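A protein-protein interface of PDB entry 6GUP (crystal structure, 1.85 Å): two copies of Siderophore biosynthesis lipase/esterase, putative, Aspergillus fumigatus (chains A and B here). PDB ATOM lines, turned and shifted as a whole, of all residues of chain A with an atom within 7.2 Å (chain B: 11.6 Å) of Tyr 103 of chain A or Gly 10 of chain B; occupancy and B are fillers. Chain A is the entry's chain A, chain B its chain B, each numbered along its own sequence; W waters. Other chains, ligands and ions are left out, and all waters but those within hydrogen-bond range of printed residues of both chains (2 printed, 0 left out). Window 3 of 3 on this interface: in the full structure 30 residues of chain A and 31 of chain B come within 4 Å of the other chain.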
ATOM      1  N   ILE A  15     -14.567   1.732  -5.027  1.00  0.00           N
ATOM      2  CA  ILE A  15     -15.352   2.965  -5.114  1.00  0.00           C
ATOM      3  C   ILE A  15     -15.765   3.388  -3.707  1.00  0.00           C
ATOM      4  O   ILE A  15     -16.374   2.601  -2.977  1.00  0.00           O
ATOM      5  CB  ILE A  15     -16.622   2.771  -5.980  1.00  0.00           C
ATOM      6  CG1 ILE A  15     -16.245   2.239  -7.372  1.00  0.00           C
ATOM      7  CG2 ILE A  15     -17.405   4.079  -6.098  1.00  0.00           C
ATOM      8  CD1 ILE A  15     -17.416   1.995  -8.303  1.00  0.00           C
ATOM      9  N   LEU A  16     -15.438   4.627  -3.337  1.00  0.00           N
ATOM     10  CA  LEU A  16     -15.881   5.206  -2.069  1.00  0.00           C
ATOM     11  C   LEU A  16     -17.197   5.954  -2.279  1.00  0.00           C
ATOM     12  O   LEU A  16     -17.250   6.929  -3.035  1.00  0.00           O
ATOM     13  CB  LEU A  16     -14.822   6.156  -1.501  1.00  0.00           C
ATOM     14  CG  LEU A  16     -15.064   6.681  -0.079  1.00  0.00           C
ATOM     15  CD1 LEU A  16     -14.991   5.555   0.945  1.00  0.00           C
ATOM     16  CD2 LEU A  16     -14.062   7.772   0.262  1.00  0.00           C
ATOM     17  N   HIS A  17     -18.249   5.485  -1.607  1.00  0.00           N
ATOM     18  CA  HIS A  17     -19.581   6.085  -1.683  1.00  0.00           C
ATOM     19  C   HIS A  17     -19.902   6.872  -0.422  1.00  0.00           C
ATOM     20  O   HIS A  17     -19.295   6.655   0.621  1.00  0.00           O
ATOM     21  CB  HIS A  17     -20.643   5.001  -1.839  1.00  0.00           C
ATOM     22  CG  HIS A  17     -20.408   4.081  -2.995  1.00  0.00           C
ATOM     23  ND1 HIS A  17     -20.995   4.271  -4.226  1.00  0.00           N
ATOM     24  CD2 HIS A  17     -19.653   2.963  -3.104  1.00  0.00           C
ATOM     25  CE1 HIS A  17     -20.611   3.311  -5.045  1.00  0.00           C
ATOM     26  NE2 HIS A  17     -19.797   2.503  -4.390  1.00  0.00           N
ATOM     27  N   GLU A  27     -16.881   0.165  -1.755  1.00  0.00           N
ATOM     28  CA  GLU A  27     -17.182  -0.980  -2.613  1.00  0.00           C
ATOM     29  C   GLU A  27     -15.887  -1.507  -3.216  1.00  0.00           C
ATOM     30  O   GLU A  27     -15.168  -0.755  -3.865  1.00  0.00           O
ATOM     31  CB  GLU A  27     -18.127  -0.556  -3.738  1.00  0.00           C
ATOM     32  CG  GLU A  27     -18.600  -1.692  -4.639  1.00  0.00           C
ATOM     33  CD  GLU A  27     -19.505  -1.232  -5.769  1.00  0.00           C
ATOM     34  OE1 GLU A  27     -19.581  -0.014  -6.044  1.00  0.00           O
ATOM     35  OE2 GLU A  27     -20.146  -2.101  -6.395  1.00  0.00           O
ATOM     36  N   THR A  29     -13.970  -3.297  -5.982  1.00  0.00           N
ATOM     37  CA  THR A  29     -14.183  -3.616  -7.393  1.00  0.00           C
ATOM     38  C   THR A  29     -12.952  -3.296  -8.233  1.00  0.00           C
ATOM     39  O   THR A  29     -12.334  -2.239  -8.074  1.00  0.00           O
ATOM     40  CB  THR A  29     -15.435  -2.907  -7.973  1.00  0.00           C
ATOM     41  OG1 THR A  29     -15.576  -3.229  -9.364  1.00  0.00           O
ATOM     42  CG2 THR A  29     -15.365  -1.388  -7.806  1.00  0.00           C
ATOM     43  N   LYS A  35     -22.669  -6.591 -11.572  1.00  0.00           N
ATOM     44  CA  LYS A  35     -22.742  -6.856 -10.133  1.00  0.00           C
ATOM     45  C   LYS A  35     -24.116  -6.458  -9.594  1.00  0.00           C
ATOM     46  O   LYS A  35     -24.224  -5.504  -8.824  1.00  0.00           O
ATOM     47  CB  LYS A  35     -21.672  -6.053  -9.383  1.00  0.00           C
ATOM     48  CG  LYS A  35     -20.239  -6.323  -9.790  1.00  0.00           C
ATOM     49  CD  LYS A  35     -19.774  -7.705  -9.384  1.00  0.00           C
ATOM     50  CE  LYS A  35     -18.289  -7.836  -9.652  1.00  0.00           C
ATOM     51  NZ  LYS A  35     -17.757  -9.204  -9.419  1.00  0.00           N
ATOM     52  N   SER A  38     -25.203  -7.666  -3.817  1.00  0.00           N
ATOM     53  CA  SER A  38     -24.384  -6.909  -2.863  1.00  0.00           C
ATOM     54  C   SER A  38     -24.197  -7.648  -1.540  1.00  0.00           C
ATOM     55  O   SER A  38     -25.161  -8.159  -0.971  1.00  0.00           O
ATOM     56  CB  SER A  38     -25.045  -5.560  -2.577  1.00  0.00           C
ATOM     57  OG  SER A  38     -25.223  -4.815  -3.766  1.00  0.00           O
ATOM     58  N   SER A  68     -20.708  -7.853  -5.450  1.00  0.00           N
ATOM     59  CA  SER A  68     -19.664  -6.899  -5.062  1.00  0.00           C
ATOM     60  C   SER A  68     -19.698  -6.705  -3.545  1.00  0.00           C
ATOM     61  O   SER A  68     -20.772  -6.651  -2.940  1.00  0.00           O
ATOM     62  CB  SER A  68     -19.831  -5.562  -5.790  1.00  0.00           C
ATOM     63  OG  SER A  68     -20.926  -4.821  -5.288  1.00  0.00           O
ATOM     64  N   PHE A  70     -19.138  -4.709  -0.037  1.00  0.00           N
ATOM     65  CA  PHE A  70     -19.136  -3.389   0.599  1.00  0.00           C
ATOM     66  C   PHE A  70     -18.699  -3.502   2.054  1.00  0.00           C
ATOM     67  O   PHE A  70     -19.027  -4.476   2.732  1.00  0.00           O
ATOM     68  CB  PHE A  70     -20.535  -2.773   0.590  1.00  0.00           C
ATOM     69  CG  PHE A  70     -21.011  -2.335  -0.762  1.00  0.00           C
ATOM     70  CD1 PHE A  70     -21.531  -3.260  -1.659  1.00  0.00           C
ATOM     71  CD2 PHE A  70     -20.975  -0.994  -1.129  1.00  0.00           C
ATOM     72  CE1 PHE A  70     -21.988  -2.860  -2.905  1.00  0.00           C
ATOM     73  CE2 PHE A  70     -21.435  -0.586  -2.373  1.00  0.00           C
ATOM     74  CZ  PHE A  70     -21.938  -1.521  -3.264  1.00  0.00           C
ATOM     75  N   LEU A  97     -27.979   0.228   3.250  1.00  0.00           N
ATOM     76  CA  LEU A  97     -28.679  -0.752   2.414  1.00  0.00           C
ATOM     77  C   LEU A  97     -29.610  -0.093   1.400  1.00  0.00           C
ATOM     78  O   LEU A  97     -29.670  -0.528   0.248  1.00  0.00           O
ATOM     79  CB  LEU A  97     -29.479  -1.734   3.274  1.00  0.00           C
ATOM     80  CG  LEU A  97     -28.680  -2.702   4.148  1.00  0.00           C
ATOM     81  CD1 LEU A  97     -29.611  -3.438   5.093  1.00  0.00           C
ATOM     82  CD2 LEU A  97     -27.915  -3.693   3.298  1.00  0.00           C
ATOM     83  N   LYS A  98     -30.334   0.941   1.831  1.00  0.00           N
ATOM     84  CA  LYS A  98     -31.181   1.725   0.925  1.00  0.00           C
ATOM     85  C   LYS A  98     -30.362   2.335  -0.205  1.00  0.00           C
ATOM     86  O   LYS A  98     -30.767   2.275  -1.368  1.00  0.00           O
ATOM     87  CB  LYS A  98     -31.925   2.842   1.667  1.00  0.00           C
ATOM     88  CG  LYS A  98     -32.826   3.664   0.751  1.00  0.00           C
ATOM     89  CD  LYS A  98     -33.460   4.854   1.439  1.00  0.00           C
ATOM     90  CE  LYS A  98     -34.341   5.606   0.453  1.00  0.00           C
ATOM     91  NZ  LYS A  98     -35.209   6.615   1.115  1.00  0.00           N
ATOM     92  N   TYR A  99     -29.225   2.931   0.149  1.00  0.00           N
ATOM     93  CA  TYR A  99     -28.328   3.533  -0.835  1.00  0.00           C
ATOM     94  C   TYR A  99     -27.804   2.505  -1.840  1.00  0.00           C
ATOM     95  O   TYR A  99     -27.850   2.740  -3.048  1.00  0.00           O
ATOM     96  CB  TYR A  99     -27.146   4.234  -0.156  1.00  0.00           C
ATOM     97  CG  TYR A  99     -26.103   4.680  -1.151  1.00  0.00           C
ATOM     98  CD1 TYR A  99     -26.269   5.856  -1.880  1.00  0.00           C
ATOM     99  CD2 TYR A  99     -24.970   3.903  -1.399  1.00  0.00           C
ATOM    100  CE1 TYR A  99     -25.325   6.260  -2.812  1.00  0.00           C
ATOM    101  CE2 TYR A  99     -24.023   4.296  -2.331  1.00  0.00           C
ATOM    102  CZ  TYR A  99     -24.202   5.476  -3.034  1.00  0.00           C
ATOM    103  OH  TYR A  99     -23.265   5.872  -3.957  1.00  0.00           O
ATOM    104  N   ILE A 100     -27.297   1.382  -1.329  1.00  0.00           N
ATOM    105  CA  ILE A 100     -26.764   0.300  -2.171  1.00  0.00           C
ATOM    106  C   ILE A 100     -27.827  -0.220  -3.139  1.00  0.00           C
ATOM    107  O   ILE A 100     -27.531  -0.484  -4.306  1.00  0.00           O
ATOM    108  CB  ILE A 100     -26.197  -0.870  -1.321  1.00  0.00           C
ATOM    109  CG1 ILE A 100     -24.895  -0.438  -0.636  1.00  0.00           C
ATOM    110  CG2 ILE A 100     -25.926  -2.107  -2.180  1.00  0.00           C
ATOM    111  CD1 ILE A 100     -24.420  -1.371   0.459  1.00  0.00           C
ATOM    112  N   LYS A 101     -29.055  -0.358  -2.644  1.00  0.00           N
ATOM    113  CA  LYS A 101     -30.171  -0.857  -3.447  1.00  0.00           C
ATOM    114  C   LYS A 101     -30.522   0.084  -4.601  1.00  0.00           C
ATOM    115  O   LYS A 101     -30.718  -0.377  -5.728  1.00  0.00           O
ATOM    116  CB  LYS A 101     -31.395  -1.104  -2.561  1.00  0.00           C
ATOM    117  CG  LYS A 101     -32.497  -1.930  -3.212  1.00  0.00           C
ATOM    118  CD  LYS A 101     -33.192  -2.827  -2.193  1.00  0.00           C
ATOM    119  CE  LYS A 101     -34.657  -3.074  -2.509  1.00  0.00           C
ATOM    120  NZ  LYS A 101     -35.338  -3.763  -1.375  1.00  0.00           N
ATOM    121  N   GLU A 102     -30.592   1.388  -4.326  1.00  0.00           N
ATOM    122  CA  GLU A 102     -30.824   2.387  -5.384  1.00  0.00           C
ATOM    123  C   GLU A 102     -29.613   2.510  -6.313  1.00  0.00           C
ATOM    124  O   GLU A 102     -29.779   2.637  -7.527  1.00  0.00           O
ATOM    125  CB  GLU A 102     -31.212   3.761  -4.799  1.00  0.00           C
ATOM    126  CG  GLU A 102     -31.191   4.952  -5.767  1.00  0.00           C
ATOM    127  CD  GLU A 102     -32.275   4.916  -6.841  1.00  0.00           C
ATOM    128  OE1 GLU A 102     -32.865   5.984  -7.111  1.00  0.00           O
ATOM    129  OE2 GLU A 102     -32.542   3.845  -7.425  1.00  0.00           O
ATOM    130  N   TYR A 103     -28.410   2.489  -5.737  1.00  0.00           N
ATOM    131  CA  TYR A 103     -27.163   2.549  -6.512  1.00  0.00           C
ATOM    132  C   TYR A 103     -27.051   1.409  -7.523  1.00  0.00           C
ATOM    133  O   TYR A 103     -26.740   1.644  -8.693  1.00  0.00           O
ATOM    134  CB  TYR A 103     -25.941   2.537  -5.580  1.00  0.00           C
ATOM    135  CG  TYR A 103     -24.635   2.189  -6.265  1.00  0.00           C
ATOM    136  CD1 TYR A 103     -24.070   3.045  -7.211  1.00  0.00           C
ATOM    137  CD2 TYR A 103     -23.962   1.001  -5.967  1.00  0.00           C
ATOM    138  CE1 TYR A 103     -22.875   2.727  -7.843  1.00  0.00           C
ATOM    139  CE2 TYR A 103     -22.766   0.677  -6.591  1.00  0.00           C
ATOM    140  CZ  TYR A 103     -22.226   1.541  -7.530  1.00  0.00           C
ATOM    141  OH  TYR A 103     -21.037   1.227  -8.146  1.00  0.00           O
ATOM    142  N   LYS A 104     -27.296   0.184  -7.061  1.00  0.00           N
ATOM    143  CA  LYS A 104     -27.216  -1.000  -7.924  1.00  0.00           C
ATOM    144  C   LYS A 104     -28.315  -1.051  -8.984  1.00  0.00           C
ATOM    145  O   LYS A 104     -28.095  -1.591 -10.072  1.00  0.00           O
ATOM    146  CB  LYS A 104     -27.212  -2.294  -7.095  1.00  0.00           C
ATOM    147  CG  LYS A 104     -25.911  -2.558  -6.347  1.00  0.00           C
ATOM    148  CD  LYS A 104     -24.733  -2.725  -7.298  1.00  0.00           C
ATOM    149  CE  LYS A 104     -23.449  -3.104  -6.580  1.00  0.00           C
ATOM    150  NZ  LYS A 104     -23.383  -4.547  -6.225  1.00  0.00           N
ATOM    151  N   THR A 105     -29.486  -0.499  -8.671  1.00  0.00           N
ATOM    152  CA  THR A 105     -30.546  -0.329  -9.664  1.00  0.00           C
ATOM    153  C   THR A 105     -30.119   0.690 -10.723  1.00  0.00           C
ATOM    154  O   THR A 105     -30.174   0.401 -11.914  1.00  0.00           O
ATOM    155  CB  THR A 105     -31.866   0.135  -9.021  1.00  0.00           C
ATOM    156  OG1 THR A 105     -32.229  -0.762  -7.965  1.00  0.00           O
ATOM    157  CG2 THR A 105     -32.993   0.180 -10.056  1.00  0.00           C
ATOM    158  N   GLU A 106     -29.701   1.873 -10.279  1.00  0.00           N
ATOM    159  CA  GLU A 106     -29.261   2.945 -11.188  1.00  0.00           C
ATOM    160  C   GLU A 106     -28.093   2.543 -12.093  1.00  0.00           C
ATOM    161  O   GLU A 106     -28.094   2.864 -13.283  1.00  0.00           O
ATOM    162  CB  GLU A 106     -28.880   4.206 -10.403  1.00  0.00           C
ATOM    163  CG  GLU A 106     -30.069   5.000  -9.889  1.00  0.00           C
ATOM    164  CD  GLU A 106     -29.659   6.262  -9.151  1.00  0.00           C
ATOM    165  OE1 GLU A 106     -30.298   7.312  -9.371  1.00  0.00           O
ATOM    166  OE2 GLU A 106     -28.698   6.210  -8.353  1.00  0.00           O
ATOM    167  N   LYS A 107     -27.107   1.844 -11.527  1.00  0.00           N
ATOM    168  CA  LYS A 107     -25.897   1.473 -12.266  1.00  0.00           C
ATOM    169  C   LYS A 107     -26.152   0.381 -13.306  1.00  0.00           C
ATOM    170  O   LYS A 107     -25.870   0.580 -14.490  1.00  0.00           O
ATOM    171  CB  LYS A 107     -24.780   1.041 -11.307  1.00  0.00           C
ATOM    172  CG  LYS A 107     -23.452   0.761 -11.999  1.00  0.00           C
ATOM    173  CD  LYS A 107     -22.282   0.805 -11.030  1.00  0.00           C
ATOM    174  CE  LYS A 107     -20.978   0.431 -11.719  1.00  0.00           C
ATOM    175  NZ  LYS A 107     -19.895   0.132 -10.743  1.00  0.00           N
ATOM    176  N   PHE A 108     -26.688  -0.756 -12.863  1.00  0.00           N
ATOM    177  CA  PHE A 108     -26.851  -1.937 -13.725  1.00  0.00           C
ATOM    178  C   PHE A 108     -28.276  -2.173 -14.243  1.00  0.00           C
ATOM    179  O   PHE A 108     -28.486  -3.085 -15.044  1.00  0.00           O
ATOM    180  CB  PHE A 108     -26.339  -3.187 -13.001  1.00  0.00           C
ATOM    181  CG  PHE A 108     -24.914  -3.074 -12.539  1.00  0.00           C
ATOM    182  CD1 PHE A 108     -23.861  -3.426 -13.380  1.00  0.00           C
ATOM    183  CD2 PHE A 108     -24.622  -2.600 -11.264  1.00  0.00           C
ATOM    184  CE1 PHE A 108     -22.544  -3.310 -12.953  1.00  0.00           C
ATOM    185  CE2 PHE A 108     -23.308  -2.487 -10.831  1.00  0.00           C
ATOM    186  CZ  PHE A 108     -22.267  -2.845 -11.675  1.00  0.00           C
ATOM    187  N   GLY A 109     -29.241  -1.361 -13.804  1.00  0.00           N
ATOM    188  CA  GLY A 109     -30.613  -1.439 -14.313  1.00  0.00           C
ATOM    189  C   GLY A 109     -31.308  -2.745 -13.975  1.00  0.00           C
ATOM    190  O   GLY A 109     -31.383  -3.132 -12.806  1.00  0.00           O
ATOM    191  N   TRP B   7     -22.076  14.518  -2.823  1.00  0.00           N
ATOM    192  CA  TRP B   7     -21.135  13.502  -3.398  1.00  0.00           C
ATOM    193  C   TRP B   7     -21.615  13.064  -4.795  1.00  0.00           C
ATOM    194  O   TRP B   7     -22.823  12.938  -5.008  1.00  0.00           O
ATOM    195  CB  TRP B   7     -20.999  12.286  -2.467  1.00  0.00           C
ATOM    196  CG  TRP B   7     -19.677  11.569  -2.549  1.00  0.00           C
ATOM    197  CD1 TRP B   7     -19.467  10.267  -2.908  1.00  0.00           C
ATOM    198  CD2 TRP B   7     -18.385  12.113  -2.250  1.00  0.00           C
ATOM    199  NE1 TRP B   7     -18.126   9.967  -2.852  1.00  0.00           N
ATOM    200  CE2 TRP B   7     -17.438  11.083  -2.454  1.00  0.00           C
ATOM    201  CE3 TRP B   7     -17.936  13.373  -1.830  1.00  0.00           C
ATOM    202  CZ2 TRP B   7     -16.066  11.272  -2.248  1.00  0.00           C
ATOM    203  CZ3 TRP B   7     -16.571  13.564  -1.629  1.00  0.00           C
ATOM    204  CH2 TRP B   7     -15.652  12.517  -1.840  1.00  0.00           C
ATOM    205  N   PRO B   8     -20.679  12.842  -5.747  1.00  0.00           N
ATOM    206  CA  PRO B   8     -21.030  12.450  -7.124  1.00  0.00           C
ATOM    207  C   PRO B   8     -21.858  11.172  -7.248  1.00  0.00           C
ATOM    208  O   PRO B   8     -21.746  10.276  -6.407  1.00  0.00           O
ATOM    209  CB  PRO B   8     -19.663  12.235  -7.782  1.00  0.00           C
ATOM    210  CG  PRO B   8     -18.751  13.125  -7.027  1.00  0.00           C
ATOM    211  CD  PRO B   8     -19.229  13.074  -5.613  1.00  0.00           C
ATOM    212  N   LYS B   9     -22.678  11.106  -8.297  1.00  0.00           N
ATOM    213  CA  LYS B   9     -23.483   9.917  -8.592  1.00  0.00           C
ATOM    214  C   LYS B   9     -22.575   8.717  -8.876  1.00  0.00           C
ATOM    215  O   LYS B   9     -21.644   8.812  -9.678  1.00  0.00           O
ATOM    216  CB  LYS B   9     -24.419  10.175  -9.785  1.00  0.00           C
ATOM    217  CG  LYS B   9     -25.043   8.929 -10.406  1.00  0.00           C
ATOM    218  CD  LYS B   9     -26.041   9.283 -11.496  1.00  0.00           C
ATOM    219  CE  LYS B   9     -26.146   8.170 -12.528  1.00  0.00           C
ATOM    220  NZ  LYS B   9     -27.271   8.388 -13.476  1.00  0.00           N
ATOM    221  N   GLY B  10     -22.861   7.600  -8.210  1.00  0.00           N
ATOM    222  CA  GLY B  10     -22.110   6.360  -8.383  1.00  0.00           C
ATOM    223  C   GLY B  10     -20.806   6.262  -7.607  1.00  0.00           C
ATOM    224  O   GLY B  10     -20.004   5.364  -7.872  1.00  0.00           O
ATOM    225  N   GLY B  11     -20.585   7.170  -6.654  1.00  0.00           N
ATOM    226  CA  GLY B  11     -19.350   7.190  -5.864  1.00  0.00           C
ATOM    227  C   GLY B  11     -18.145   7.643  -6.668  1.00  0.00           C
ATOM    228  O   GLY B  11     -18.277   8.025  -7.836  1.00  0.00           O
ATOM    229  N   LEU B  12     -16.970   7.599  -6.042  1.00  0.00           N
ATOM    230  CA  LEU B  12     -15.724   7.978  -6.703  1.00  0.00           C
ATOM    231  C   LEU B  12     -14.696   6.851  -6.635  1.00  0.00           C
ATOM    232  O   LEU B  12     -14.404   6.347  -5.547  1.00  0.00           O
ATOM    233  CB  LEU B  12     -15.164   9.267  -6.097  1.00  0.00           C
ATOM    234  CG  LEU B  12     -15.969  10.534  -6.412  1.00  0.00           C
ATOM    235  CD1 LEU B  12     -15.312  11.741  -5.765  1.00  0.00           C
ATOM    236  CD2 LEU B  12     -16.111  10.748  -7.917  1.00  0.00           C
ATOM    237  N   PRO B  13     -14.145   6.449  -7.802  1.00  0.00           N
ATOM    238  CA  PRO B  13     -13.227   5.316  -7.842  1.00  0.00           C
ATOM    239  C   PRO B  13     -11.857   5.645  -7.258  1.00  0.00           C
ATOM    240  O   PRO B  13     -11.417   6.796  -7.302  1.00  0.00           O
ATOM    241  CB  PRO B  13     -13.116   5.012  -9.338  1.00  0.00           C
ATOM    242  CG  PRO B  13     -13.309   6.334  -9.989  1.00  0.00           C
ATOM    243  CD  PRO B  13     -14.318   7.052  -9.140  1.00  0.00           C
ATOM    244  N   GLY B  14     -11.198   4.629  -6.716  1.00  0.00           N
ATOM    245  CA  GLY B  14      -9.887   4.807  -6.113  1.00  0.00           C
ATOM    246  C   GLY B  14      -9.321   3.533  -5.523  1.00  0.00           C
ATOM    247  O   GLY B  14      -9.724   2.433  -5.903  1.00  0.00           O
ATOM    248  N   PHE B  26      -7.446   6.585   1.687  1.00  0.00           N
ATOM    249  CA  PHE B  26      -8.085   6.351   0.397  1.00  0.00           C
ATOM    250  C   PHE B  26      -7.432   7.226  -0.666  1.00  0.00           C
ATOM    251  O   PHE B  26      -7.356   8.446  -0.506  1.00  0.00           O
ATOM    252  CB  PHE B  26      -9.579   6.653   0.463  1.00  0.00           C
ATOM    253  CG  PHE B  26     -10.309   6.338  -0.811  1.00  0.00           C
ATOM    254  CD1 PHE B  26     -10.607   5.023  -1.145  1.00  0.00           C
ATOM    255  CD2 PHE B  26     -10.683   7.352  -1.689  1.00  0.00           C
ATOM    256  CE1 PHE B  26     -11.274   4.725  -2.325  1.00  0.00           C
ATOM    257  CE2 PHE B  26     -11.350   7.059  -2.870  1.00  0.00           C
ATOM    258  CZ  PHE B  26     -11.647   5.743  -3.187  1.00  0.00           C
ATOM    259  N   TYR B  28      -7.561   8.751  -4.371  1.00  0.00           N
ATOM    260  CA  TYR B  28      -8.356   9.084  -5.553  1.00  0.00           C
ATOM    261  C   TYR B  28      -7.419   9.078  -6.743  1.00  0.00           C
ATOM    262  O   TYR B  28      -6.461   9.855  -6.786  1.00  0.00           O
ATOM    263  CB  TYR B  28      -8.992  10.465  -5.434  1.00  0.00           C
ATOM    264  CG  TYR B  28      -9.994  10.587  -4.320  1.00  0.00           C
ATOM    265  CD1 TYR B  28      -9.588  10.871  -3.016  1.00  0.00           C
ATOM    266  CD2 TYR B  28     -11.357  10.428  -4.565  1.00  0.00           C
ATOM    267  CE1 TYR B  28     -10.511  10.988  -1.987  1.00  0.00           C
ATOM    268  CE2 TYR B  28     -12.286  10.542  -3.545  1.00  0.00           C
ATOM    269  CZ  TYR B  28     -11.861  10.820  -2.260  1.00  0.00           C
ATOM    270  OH  TYR B  28     -12.792  10.929  -1.258  1.00  0.00           O
ATOM    271  N   ALA B  56     -14.486  16.152  -3.914  1.00  0.00           N
ATOM    272  CA  ALA B  56     -14.903  15.563  -5.188  1.00  0.00           C
ATOM    273  C   ALA B  56     -14.392  16.371  -6.384  1.00  0.00           C
ATOM    274  O   ALA B  56     -13.918  15.798  -7.367  1.00  0.00           O
ATOM    275  CB  ALA B  56     -16.417  15.441  -5.243  1.00  0.00           C
ATOM    276  N   HIS B  60     -11.445  15.087  -9.025  1.00  0.00           N
ATOM    277  CA  HIS B  60     -11.731  15.106 -10.465  1.00  0.00           C
ATOM    278  C   HIS B  60     -10.739  15.975 -11.248  1.00  0.00           C
ATOM    279  O   HIS B  60     -10.331  15.611 -12.354  1.00  0.00           O
ATOM    280  CB  HIS B  60     -13.163  15.580 -10.732  1.00  0.00           C
ATOM    281  CG  HIS B  60     -13.632  15.304 -12.126  1.00  0.00           C
ATOM    282  ND1 HIS B  60     -13.390  16.165 -13.175  1.00  0.00           N
ATOM    283  CD2 HIS B  60     -14.313  14.256 -12.648  1.00  0.00           C
ATOM    284  CE1 HIS B  60     -13.910  15.662 -14.282  1.00  0.00           C
ATOM    285  NE2 HIS B  60     -14.475  14.505 -13.989  1.00  0.00           N
ATOM    286  N   GLN B  63      -7.296  14.240 -11.992  1.00  0.00           N
ATOM    287  CA  GLN B  63      -7.319  13.048 -12.861  1.00  0.00           C
ATOM    288  C   GLN B  63      -6.408  13.117 -14.100  1.00  0.00           C
ATOM    289  O   GLN B  63      -5.714  12.141 -14.392  1.00  0.00           O
ATOM    290  CB  GLN B  63      -8.756  12.694 -13.282  1.00  0.00           C
ATOM    291  CG  GLN B  63      -9.626  12.206 -12.133  1.00  0.00           C
ATOM    292  CD  GLN B  63     -10.963  11.647 -12.582  1.00  0.00           C
ATOM    293  OE1 GLN B  63     -11.475  11.991 -13.649  1.00  0.00           O
ATOM    294  NE2 GLN B  63     -11.545  10.783 -11.757  1.00  0.00           N
HETATM  295  O   HOH W   1     -20.108   3.633  -9.968  1.00  0.00           O
HETATM  296  O   HOH W   2     -24.523   7.077  -6.071  1.00  0.00           O
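No position is printed for both chains.
Of the 11 pairs that touch across the chains among the printed residues, none has its exchanged pair printed and touching as well.
Among the printed residues, merely in contact across the chains: Ile 15 of chain A with Gly 10 of chain B (3.4 Å), Ile 15 of chain A with Gly 11 of chain B (3.7 Å), Ile 15 of chain A with Leu 12 of chain B (3.5 Å), Leu 16 of chain A with Gly 11 of chain B (3.5 Å), Leu 16 of chain A with Phe 26 of chain B (3.6 Å), Leu 16 of chain A with Tyr 28 of chain B (3.7 Å), His 17 of chain A with Gly 10 of chain B (3.5 Å), His 17 of chain A with Gly 11 of chain B (3.7 Å) and Tyr 103 of chain A with Gly 10 of chain B (3.8 Å).
O of Ile 15 of chain A sits at hydrogen-bond distance from N of Glu 27 of chain A (2.8 Å).
A ring nitrogen (NE2) of His 17 of chain A lies within hydrogen-bond range of the side-chain carboxylate (OE1) of Glu 27 of chain A, at 3.0 Å.
OH of Tyr 99 of chain A sits at hydrogen-bond distance from ND1 of His 17 of chain A (2.8 Å).
The side-chain carboxylate (OE1) of Glu 27 of chain A lies within hydrogen-bond range of the side-chain hydroxyl (OH) of Tyr 103 of chain A, at 2.8 Å.
OH of Tyr 103 of chain A lies within hydrogen-bond range of NZ of Lys 107 of chain A (3.0 Å).
Of chain B, only Gly 10 (3.4 Å), Gly 11 (3.7 Å) and Leu 12 (3.5 Å) come within 4 Å of Ile 15 of chain A.
Of the printed residues of chain B, Leu 16 of chain A touches Trp 7, Gly 11, Leu 12, Phe 26 and Tyr 28.
Ile 100 of chain A touches none of the printed residues of chain B.
Glu 102 of chain A touches none of the printed residues of chain B.
Tyr 103 of chain A touches just one residue of chain B: Gly 10.
No residue of chain B comes within 4 Å of Lys 104 of chain A.
No residue of chain B comes within 4 Å of Thr 105 of chain A.
No residue of chain B comes within 4 Å of Glu 106 of chain A.
Of the printed residues of chain A, Trp 7 of chain B touches Leu 16 (3.2 Å).
Gly 10 of chain B touches just these residues of chain A: Ile 15, His 17 and Tyr 103.
Of the printed residues of chain A, Gly 11 of chain B touches Ile 15, Leu 16 and His 17.
Of the printed residues of chain A, Phe 26 of chain B touches Leu 16 (3.6 Å).
Printed residues of chain A within 4 Å of Tyr 28 of chain B: Leu 16 (3.7 Å).
The nearest residue of chain B that does not touch Tyr 103 of chain A is Gly 11 of chain B (5.1 Å).
The nearest printed residue of chain A that does not touch Trp 7 of chain B is His 17 of chain A (4.2 Å).
Of the 13 printed residues of chain B, 6 touch a printed residue of chain A.
Of the 22 printed residues of chain A, 4 touch a printed residue of chain B.
Among the printed residues, no Asp or Glu carboxylate lies within 4 Å of a Lys or Arg side-chain nitrogen of the other chain.
Water W1 bridges O of Gly 10 of chain B (2.7 Å) and OH of Tyr 103 of chain A (3.2 Å).
Water W2 lies within hydrogen-bond range of OH of Tyr 99 of chain A (2.7 Å) and N of Gly 10 of chain B (2.8 Å).
The indole nitrogen (NE1) of Trp 7 of chain B sits at hydrogen-bond distance from the backbone carbonyl oxygen (O) of Leu 16 of chain A (3.2 Å).
The backbone NH (N) of Leu 16 of chain A sits at hydrogen-bond distance from the backbone carbonyl oxygen (O) of Leu 12 of chain B (3.0 Å).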
